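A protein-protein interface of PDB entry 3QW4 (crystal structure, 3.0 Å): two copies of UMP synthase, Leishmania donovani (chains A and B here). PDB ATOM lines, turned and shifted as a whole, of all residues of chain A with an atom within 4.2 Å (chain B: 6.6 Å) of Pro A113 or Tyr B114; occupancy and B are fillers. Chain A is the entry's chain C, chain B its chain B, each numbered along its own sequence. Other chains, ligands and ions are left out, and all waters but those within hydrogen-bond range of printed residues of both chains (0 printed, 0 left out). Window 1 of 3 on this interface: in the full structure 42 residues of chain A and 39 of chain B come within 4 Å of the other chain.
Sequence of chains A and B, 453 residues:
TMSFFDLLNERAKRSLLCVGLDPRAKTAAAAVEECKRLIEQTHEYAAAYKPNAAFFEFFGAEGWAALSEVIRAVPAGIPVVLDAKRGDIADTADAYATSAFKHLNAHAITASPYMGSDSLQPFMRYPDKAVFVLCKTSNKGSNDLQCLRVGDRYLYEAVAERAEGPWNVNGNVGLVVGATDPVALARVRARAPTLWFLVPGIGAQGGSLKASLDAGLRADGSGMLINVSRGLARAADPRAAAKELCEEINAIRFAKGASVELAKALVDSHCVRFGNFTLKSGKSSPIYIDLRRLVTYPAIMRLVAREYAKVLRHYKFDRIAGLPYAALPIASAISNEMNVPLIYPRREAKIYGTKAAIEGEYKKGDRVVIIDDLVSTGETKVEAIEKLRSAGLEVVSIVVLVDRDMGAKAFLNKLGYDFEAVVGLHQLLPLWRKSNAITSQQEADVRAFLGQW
Printed residues of chain A that touch a printed residue of chain B: Pro A113, Tyr A114, Met A115, Gly A116, Leu A134, Cys A135, Leu A145, Gln A146, Leu A155, Tyr A156 and Val A159. Of the 13 printed residues of chain B, 6 touch a printed residue of chain A. Printed residues of chain B that touch a printed residue of chain A: Pro B113, Tyr B114, Met B115, Gly B141, Leu B145 and Gln B146. Hydrophobic or aromatic side chains of chain B that line the printed part of chain A: Pro B113, Tyr B114 and Leu B145. Among the printed residues, 17 pairs touch across the chains. Among the printed residues, no Asp or Glu carboxylate lies within 4 Å of a Lys or Arg side-chain nitrogen of the other chain.
Among the printed residues, merely in contact across the chains: Pro A113 with Tyr B114, Pro A113 with Leu B145, Tyr A114 with Pro B113, Tyr A114 with Leu B145, Met A115 with Gly B141, Met A115 with Gln B146, Gly A116 with Gly B141, Leu A134 with Tyr B114, Leu A145 with Pro B113, Leu A145 with Tyr B114, Gln A146 with Met B115, Leu A155 with Tyr B114, Tyr A156 with Tyr B114 and Val A159 with Tyr B114.
The side-chain hydroxyl of Ser B119 lies close to the backbone carbonyl oxygen of Met B115, 3.4 Å away. The backbone NH (N) of Leu A134 lies within hydrogen-bond range of the backbone carbonyl oxygen (O) of Ala A111, 3.0 Å away. O of Cys A135 lies close to OE1 of Gln A146 (3.4 Å). SG of Cys A135 sits at hydrogen-bond distance from O of Tyr A156. The backbone carbonyl oxygen (O) of Gln A146 lies within hydrogen-bond range of the backbone NH (N) of Leu A155, at 3.2 Å. The backbone carbonyl oxygen (O) of Gln A146 sits close to the backbone NH (N) of Tyr A156, at 3.3 Å.
Pro A113 touches Tyr B114, and with the chains exchanged Tyr A114 touches Pro B113. Tyr A114 touches Leu B145, and with the chains exchanged Leu A145 touches Tyr B114. Tyr A114 touches Gln B146, and with the chains exchanged Gln A146 touches Tyr B114. Met A115 touches Gln B146, and with the chains exchanged Gln A146 touches Met B115. 9 positions are printed for both chains.
Printed residues of chain B within 4 Å of Pro A113: Tyr B114 and Leu B145. Of the printed residues of chain B, Met A115 touches Gly B141 and Gln B146. Of the printed residues of chain B, Leu A134 touches Tyr B114 (3.6 Å). Of the printed residues of chain B, Leu A145 touches Pro B113 (3.7 Å) and Tyr B114 (3.9 Å). Printed residues of chain B within 4 Å of Tyr A156: Tyr B114 (3.9 Å). Ala B111 touches none of the printed residues of chain A. Ser B112 touches none of the printed residues of chain A. Of chain A, only Pro A113, Leu A134, Cys A135, Leu A145, Gln A146, Leu A155, Tyr A156 and Val A159 come within 4 Å of Tyr B114. The nearest printed residue of chain A that does not touch Tyr B114 is Ser A112 (4.8 Å).
The backbone carbonyl oxygen of Cys A135 is in hydrogen-bond range of the side-chain hydroxyl of Tyr B114, at 2.6 Å. NE2 of Gln A146 sits at hydrogen-bond distance from O of Tyr B114, 2.9 Å away. The side-chain amide nitrogen (NE2) of Gln B146 lies within hydrogen-bond range of the backbone carbonyl oxygen (O) of Tyr A114 (3.2 Å).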
ATOM      1  N   ALA A 111     -28.026  21.147  -5.027  1.00  0.00           N
ATOM      2  CA  ALA A 111     -27.810  19.728  -4.717  1.00  0.00           C
ATOM      3  C   ALA A 111     -26.819  19.479  -3.561  1.00  0.00           C
ATOM      4  O   ALA A 111     -25.987  20.331  -3.245  1.00  0.00           O
ATOM      5  CB  ALA A 111     -27.375  18.976  -5.973  1.00  0.00           C
ATOM      6  N   SER A 112     -26.921  18.309  -2.931  1.00  0.00           N
ATOM      7  CA  SER A 112     -26.042  17.942  -1.816  1.00  0.00           C
ATOM      8  C   SER A 112     -24.833  17.165  -2.301  1.00  0.00           C
ATOM      9  O   SER A 112     -24.973  16.242  -3.106  1.00  0.00           O
ATOM     10  CB  SER A 112     -26.793  17.122  -0.763  1.00  0.00           C
ATOM     11  OG  SER A 112     -25.914  16.272  -0.032  1.00  0.00           O
ATOM     12  N   PRO A 113     -23.639  17.531  -1.799  1.00  0.00           N
ATOM     13  CA  PRO A 113     -22.415  16.825  -2.138  1.00  0.00           C
ATOM     14  C   PRO A 113     -22.324  15.440  -1.517  1.00  0.00           C
ATOM     15  O   PRO A 113     -21.557  14.617  -1.999  1.00  0.00           O
ATOM     16  CB  PRO A 113     -21.332  17.714  -1.537  1.00  0.00           C
ATOM     17  CG  PRO A 113     -22.001  18.467  -0.466  1.00  0.00           C
ATOM     18  CD  PRO A 113     -23.381  18.695  -0.930  1.00  0.00           C
ATOM     19  N   TYR A 114     -23.119  15.185  -0.477  1.00  0.00           N
ATOM     20  CA  TYR A 114     -22.885  14.065   0.441  1.00  0.00           C
ATOM     21  C   TYR A 114     -22.746  12.708  -0.219  1.00  0.00           C
ATOM     22  O   TYR A 114     -21.845  11.934   0.118  1.00  0.00           O
ATOM     23  CB  TYR A 114     -23.956  14.000   1.531  1.00  0.00           C
ATOM     24  CG  TYR A 114     -23.576  13.075   2.671  1.00  0.00           C
ATOM     25  CD1 TYR A 114     -24.195  11.843   2.831  1.00  0.00           C
ATOM     26  CD2 TYR A 114     -22.589  13.436   3.585  1.00  0.00           C
ATOM     27  CE1 TYR A 114     -23.844  10.998   3.878  1.00  0.00           C
ATOM     28  CE2 TYR A 114     -22.231  12.602   4.628  1.00  0.00           C
ATOM     29  CZ  TYR A 114     -22.857  11.385   4.772  1.00  0.00           C
ATOM     30  OH  TYR A 114     -22.497  10.559   5.809  1.00  0.00           O
ATOM     31  N   MET A 115     -23.630  12.428  -1.164  1.00  0.00           N
ATOM     32  CA  MET A 115     -23.666  11.110  -1.768  1.00  0.00           C
ATOM     33  C   MET A 115     -22.641  10.912  -2.888  1.00  0.00           C
ATOM     34  O   MET A 115     -22.729   9.966  -3.667  1.00  0.00           O
ATOM     35  CB  MET A 115     -25.093  10.762  -2.197  1.00  0.00           C
ATOM     36  CG  MET A 115     -25.999  10.407  -1.018  1.00  0.00           C
ATOM     37  SD  MET A 115     -27.697  10.002  -1.448  1.00  0.00           S
ATOM     38  CE  MET A 115     -27.489   8.390  -2.175  1.00  0.00           C
ATOM     39  N   GLY A 116     -21.652  11.793  -2.947  1.00  0.00           N
ATOM     40  CA  GLY A 116     -20.569  11.659  -3.906  1.00  0.00           C
ATOM     41  C   GLY A 116     -20.931  12.234  -5.254  1.00  0.00           C
ATOM     42  O   GLY A 116     -22.015  12.793  -5.417  1.00  0.00           O
ATOM     43  N   VAL A 133     -23.642  23.077  -5.974  1.00  0.00           N
ATOM     44  CA  VAL A 133     -23.448  22.133  -4.879  1.00  0.00           C
ATOM     45  C   VAL A 133     -23.344  22.895  -3.568  1.00  0.00           C
ATOM     46  O   VAL A 133     -22.771  23.985  -3.523  1.00  0.00           O
ATOM     47  CB  VAL A 133     -22.174  21.291  -5.078  1.00  0.00           C
ATOM     48  CG1 VAL A 133     -21.977  20.328  -3.939  1.00  0.00           C
ATOM     49  CG2 VAL A 133     -22.238  20.526  -6.383  1.00  0.00           C
ATOM     50  N   LEU A 134     -23.908  22.333  -2.503  1.00  0.00           N
ATOM     51  CA  LEU A 134     -23.828  22.970  -1.200  1.00  0.00           C
ATOM     52  C   LEU A 134     -22.400  22.869  -0.699  1.00  0.00           C
ATOM     53  O   LEU A 134     -21.795  21.799  -0.736  1.00  0.00           O
ATOM     54  CB  LEU A 134     -24.804  22.337  -0.216  1.00  0.00           C
ATOM     55  CG  LEU A 134     -26.289  22.318  -0.589  1.00  0.00           C
ATOM     56  CD1 LEU A 134     -27.093  21.654   0.510  1.00  0.00           C
ATOM     57  CD2 LEU A 134     -26.844  23.707  -0.868  1.00  0.00           C
ATOM     58  N   CYS A 135     -21.850  23.998  -0.280  1.00  0.00           N
ATOM     59  CA  CYS A 135     -20.491  24.037   0.206  1.00  0.00           C
ATOM     60  C   CYS A 135     -20.518  24.385   1.688  1.00  0.00           C
ATOM     61  O   CYS A 135     -20.511  23.494   2.545  1.00  0.00           O
ATOM     62  CB  CYS A 135     -19.679  25.060  -0.585  1.00  0.00           C
ATOM     63  SG  CYS A 135     -17.910  24.969  -0.302  1.00  0.00           S
ATOM     64  N   LEU A 145     -20.902  20.103  10.932  1.00  0.00           N
ATOM     65  CA  LEU A 145     -20.325  19.054  10.106  1.00  0.00           C
ATOM     66  C   LEU A 145     -19.323  19.594   9.096  1.00  0.00           C
ATOM     67  O   LEU A 145     -18.294  18.974   8.856  1.00  0.00           O
ATOM     68  CB  LEU A 145     -21.421  18.278   9.379  1.00  0.00           C
ATOM     69  CG  LEU A 145     -21.132  16.804   9.091  1.00  0.00           C
ATOM     70  CD1 LEU A 145     -21.691  15.949  10.205  1.00  0.00           C
ATOM     71  CD2 LEU A 145     -21.716  16.372   7.765  1.00  0.00           C
ATOM     72  N   GLN A 146     -19.624  20.750   8.513  1.00  0.00           N
ATOM     73  CA  GLN A 146     -18.807  21.322   7.442  1.00  0.00           C
ATOM     74  C   GLN A 146     -17.427  21.783   7.880  1.00  0.00           C
ATOM     75  O   GLN A 146     -16.490  21.775   7.089  1.00  0.00           O
ATOM     76  CB  GLN A 146     -19.544  22.474   6.774  1.00  0.00           C
ATOM     77  CG  GLN A 146     -20.804  22.046   6.069  1.00  0.00           C
ATOM     78  CD  GLN A 146     -21.814  23.153   5.971  1.00  0.00           C
ATOM     79  OE1 GLN A 146     -21.465  24.300   5.742  1.00  0.00           O
ATOM     80  NE2 GLN A 146     -23.083  22.814   6.146  1.00  0.00           N
ATOM     81  N   LEU A 155     -13.943  20.506   5.731  1.00  0.00           N
ATOM     82  CA  LEU A 155     -14.715  19.637   4.848  1.00  0.00           C
ATOM     83  C   LEU A 155     -15.234  20.381   3.618  1.00  0.00           C
ATOM     84  O   LEU A 155     -15.112  19.890   2.501  1.00  0.00           O
ATOM     85  CB  LEU A 155     -15.870  18.963   5.606  1.00  0.00           C
ATOM     86  CG  LEU A 155     -16.876  18.135   4.801  1.00  0.00           C
ATOM     87  CD1 LEU A 155     -16.291  16.800   4.413  1.00  0.00           C
ATOM     88  CD2 LEU A 155     -18.138  17.944   5.590  1.00  0.00           C
ATOM     89  N   TYR A 156     -15.803  21.565   3.823  1.00  0.00           N
ATOM     90  CA  TYR A 156     -16.320  22.356   2.706  1.00  0.00           C
ATOM     91  C   TYR A 156     -15.232  22.687   1.689  1.00  0.00           C
ATOM     92  O   TYR A 156     -15.512  22.800   0.500  1.00  0.00           O
ATOM     93  CB  TYR A 156     -17.031  23.630   3.191  1.00  0.00           C
ATOM     94  CG  TYR A 156     -16.180  24.614   3.984  1.00  0.00           C
ATOM     95  CD1 TYR A 156     -16.119  24.554   5.376  1.00  0.00           C
ATOM     96  CD2 TYR A 156     -15.466  25.624   3.340  1.00  0.00           C
ATOM     97  CE1 TYR A 156     -15.353  25.463   6.106  1.00  0.00           C
ATOM     98  CE2 TYR A 156     -14.688  26.543   4.061  1.00  0.00           C
ATOM     99  CZ  TYR A 156     -14.635  26.454   5.443  1.00  0.00           C
ATOM    100  OH  TYR A 156     -13.873  27.354   6.153  1.00  0.00           O
ATOM    101  N   VAL A 159     -14.769  19.807  -0.444  1.00  0.00           N
ATOM    102  CA  VAL A 159     -15.879  19.880  -1.384  1.00  0.00           C
ATOM    103  C   VAL A 159     -15.538  20.837  -2.516  1.00  0.00           C
ATOM    104  O   VAL A 159     -15.651  20.494  -3.697  1.00  0.00           O
ATOM    105  CB  VAL A 159     -17.174  20.326  -0.680  1.00  0.00           C
ATOM    106  CG1 VAL A 159     -18.254  20.683  -1.685  1.00  0.00           C
ATOM    107  CG2 VAL A 159     -17.668  19.226   0.226  1.00  0.00           C
ATOM    108  N   ALA B 111     -33.123  12.147   5.506  1.00  0.00           N
ATOM    109  CA  ALA B 111     -32.525  13.481   5.516  1.00  0.00           C
ATOM    110  C   ALA B 111     -31.001  13.454   5.369  1.00  0.00           C
ATOM    111  O   ALA B 111     -30.357  12.479   5.757  1.00  0.00           O
ATOM    112  CB  ALA B 111     -32.908  14.202   6.802  1.00  0.00           C
ATOM    113  N   SER B 112     -30.442  14.536   4.820  1.00  0.00           N
ATOM    114  CA  SER B 112     -28.997  14.716   4.702  1.00  0.00           C
ATOM    115  C   SER B 112     -28.452  15.329   5.983  1.00  0.00           C
ATOM    116  O   SER B 112     -29.109  16.185   6.579  1.00  0.00           O
ATOM    117  CB  SER B 112     -28.652  15.620   3.519  1.00  0.00           C
ATOM    118  N   PRO B 113     -27.251  14.891   6.416  1.00  0.00           N
ATOM    119  CA  PRO B 113     -26.587  15.444   7.605  1.00  0.00           C
ATOM    120  C   PRO B 113     -25.743  16.709   7.334  1.00  0.00           C
ATOM    121  O   PRO B 113     -25.277  17.364   8.276  1.00  0.00           O
ATOM    122  CB  PRO B 113     -25.672  14.304   8.036  1.00  0.00           C
ATOM    123  CG  PRO B 113     -25.361  13.580   6.766  1.00  0.00           C
ATOM    124  CD  PRO B 113     -26.526  13.728   5.867  1.00  0.00           C
ATOM    125  N   TYR B 114     -25.565  17.049   6.062  1.00  0.00           N
ATOM    126  CA  TYR B 114     -24.570  18.022   5.662  1.00  0.00           C
ATOM    127  C   TYR B 114     -24.765  19.386   6.305  1.00  0.00           C
ATOM    128  O   TYR B 114     -23.784  20.059   6.647  1.00  0.00           O
ATOM    129  CB  TYR B 114     -24.539  18.147   4.141  1.00  0.00           C
ATOM    130  CG  TYR B 114     -23.330  18.882   3.634  1.00  0.00           C
ATOM    131  CD1 TYR B 114     -23.416  20.210   3.250  1.00  0.00           C
ATOM    132  CD2 TYR B 114     -22.093  18.249   3.550  1.00  0.00           C
ATOM    133  CE1 TYR B 114     -22.297  20.896   2.788  1.00  0.00           C
ATOM    134  CE2 TYR B 114     -20.961  18.924   3.083  1.00  0.00           C
ATOM    135  CZ  TYR B 114     -21.067  20.247   2.703  1.00  0.00           C
ATOM    136  OH  TYR B 114     -19.951  20.924   2.248  1.00  0.00           O
ATOM    137  N   MET B 115     -26.016  19.793   6.493  1.00  0.00           N
ATOM    138  CA  MET B 115     -26.282  21.141   6.989  1.00  0.00           C
ATOM    139  C   MET B 115     -26.273  21.274   8.518  1.00  0.00           C
ATOM    140  O   MET B 115     -26.606  22.331   9.059  1.00  0.00           O
ATOM    141  CB  MET B 115     -27.560  21.704   6.373  1.00  0.00           C
ATOM    142  CG  MET B 115     -27.394  22.041   4.911  1.00  0.00           C
ATOM    143  SD  MET B 115     -28.714  23.033   4.185  1.00  0.00           S
ATOM    144  CE  MET B 115     -28.714  24.455   5.271  1.00  0.00           C
ATOM    145  N   GLY B 116     -25.868  20.211   9.211  1.00  0.00           N
ATOM    146  CA  GLY B 116     -25.719  20.262  10.664  1.00  0.00           C
ATOM    147  C   GLY B 116     -27.020  20.034  11.393  1.00  0.00           C
ATOM    148  O   GLY B 116     -28.041  19.757  10.760  1.00  0.00           O
ATOM    149  N   SER B 119     -30.409  22.176  11.125  1.00  0.00           N
ATOM    150  CA  SER B 119     -31.161  21.930   9.897  1.00  0.00           C
ATOM    151  C   SER B 119     -32.055  20.703  10.038  1.00  0.00           C
ATOM    152  O   SER B 119     -33.076  20.580   9.354  1.00  0.00           O
ATOM    153  CB  SER B 119     -30.216  21.756   8.715  1.00  0.00           C
ATOM    154  OG  SER B 119     -29.496  20.543   8.810  1.00  0.00           O
ATOM    155  N   LEU B 120     -31.656  19.801  10.932  1.00  0.00           N
ATOM    156  CA  LEU B 120     -32.404  18.582  11.198  1.00  0.00           C
ATOM    157  C   LEU B 120     -33.416  18.772  12.311  1.00  0.00           C
ATOM    158  O   LEU B 120     -34.365  18.003  12.408  1.00  0.00           O
ATOM    159  CB  LEU B 120     -31.456  17.440  11.553  1.00  0.00           C
ATOM    160  CG  LEU B 120     -30.446  17.042  10.471  1.00  0.00           C
ATOM    161  CD1 LEU B 120     -29.271  16.290  11.067  1.00  0.00           C
ATOM    162  CD2 LEU B 120     -31.104  16.223   9.355  1.00  0.00           C
ATOM    163  N   VAL B 133     -31.070   9.754   9.088  1.00  0.00           N
ATOM    164  CA  VAL B 133     -29.979  10.554   8.533  1.00  0.00           C
ATOM    165  C   VAL B 133     -29.117   9.686   7.592  1.00  0.00           C
ATOM    166  O   VAL B 133     -28.840   8.510   7.891  1.00  0.00           O
ATOM    167  CB  VAL B 133     -29.099  11.133   9.676  1.00  0.00           C
ATOM    168  CG1 VAL B 133     -28.096  12.100   9.151  1.00  0.00           C
ATOM    169  CG2 VAL B 133     -29.965  11.819  10.716  1.00  0.00           C
ATOM    170  N   GLY B 141     -20.073   5.703  -5.190  1.00  0.00           N
ATOM    171  CA  GLY B 141     -19.566   7.050  -4.943  1.00  0.00           C
ATOM    172  C   GLY B 141     -19.712   7.530  -3.500  1.00  0.00           C
ATOM    173  O   GLY B 141     -19.403   8.679  -3.184  1.00  0.00           O
ATOM    174  N   LEU B 145     -16.593  10.670  -0.623  1.00  0.00           N
ATOM    175  CA  LEU B 145     -16.667  11.786   0.317  1.00  0.00           C
ATOM    176  C   LEU B 145     -16.874  11.322   1.750  1.00  0.00           C
ATOM    177  O   LEU B 145     -16.286  11.871   2.676  1.00  0.00           O
ATOM    178  CB  LEU B 145     -17.774  12.771  -0.086  1.00  0.00           C
ATOM    179  CG  LEU B 145     -17.749  14.160   0.570  1.00  0.00           C
ATOM    180  CD1 LEU B 145     -16.673  15.045  -0.043  1.00  0.00           C
ATOM    181  CD2 LEU B 145     -19.092  14.843   0.468  1.00  0.00           C
ATOM    182  N   GLN B 146     -17.713  10.305   1.923  1.00  0.00           N
ATOM    183  CA  GLN B 146     -18.017   9.748   3.235  1.00  0.00           C
ATOM    184  C   GLN B 146     -16.830   8.996   3.801  1.00  0.00           C
ATOM    185  O   GLN B 146     -16.740   8.803   5.002  1.00  0.00           O
ATOM    186  CB  GLN B 146     -19.223   8.826   3.145  1.00  0.00           C
ATOM    187  CG  GLN B 146     -20.425   9.497   2.509  1.00  0.00           C
ATOM    188  CD  GLN B 146     -21.524   8.528   2.105  1.00  0.00           C
ATOM    189  OE1 GLN B 146     -21.554   7.385   2.552  1.00  0.00           O
ATOM    190  NE2 GLN B 146     -22.438   8.984   1.257  1.00  0.00           N
ATOM    191  N   TRP B 167     -27.621  14.590  18.567  1.00  0.00           N
ATOM    192  CA  TRP B 167     -28.836  14.756  17.779  1.00  0.00           C
ATOM    193  C   TRP B 167     -30.023  13.958  18.305  1.00  0.00           C
ATOM    194  O   TRP B 167     -31.174  14.375  18.133  1.00  0.00           O
ATOM    195  CB  TRP B 167     -28.589  14.394  16.320  1.00  0.00           C
ATOM    196  CG  TRP B 167     -27.550  15.230  15.636  1.00  0.00           C
ATOM    197  CD1 TRP B 167     -26.934  16.334  16.124  1.00  0.00           C
ATOM    198  CD2 TRP B 167     -27.049  15.044  14.309  1.00  0.00           C
ATOM    199  NE1 TRP B 167     -26.059  16.844  15.195  1.00  0.00           N
ATOM    200  CE2 TRP B 167     -26.116  16.073  14.068  1.00  0.00           C
ATOM    201  CE3 TRP B 167     -27.298  14.105  13.300  1.00  0.00           C
ATOM    202  CZ2 TRP B 167     -25.430  16.193  12.861  1.00  0.00           C
ATOM    203  CZ3 TRP B 167     -26.622  14.217  12.106  1.00  0.00           C
ATOM    204  CH2 TRP B 167     -25.696  15.260  11.891  1.00  0.00           C
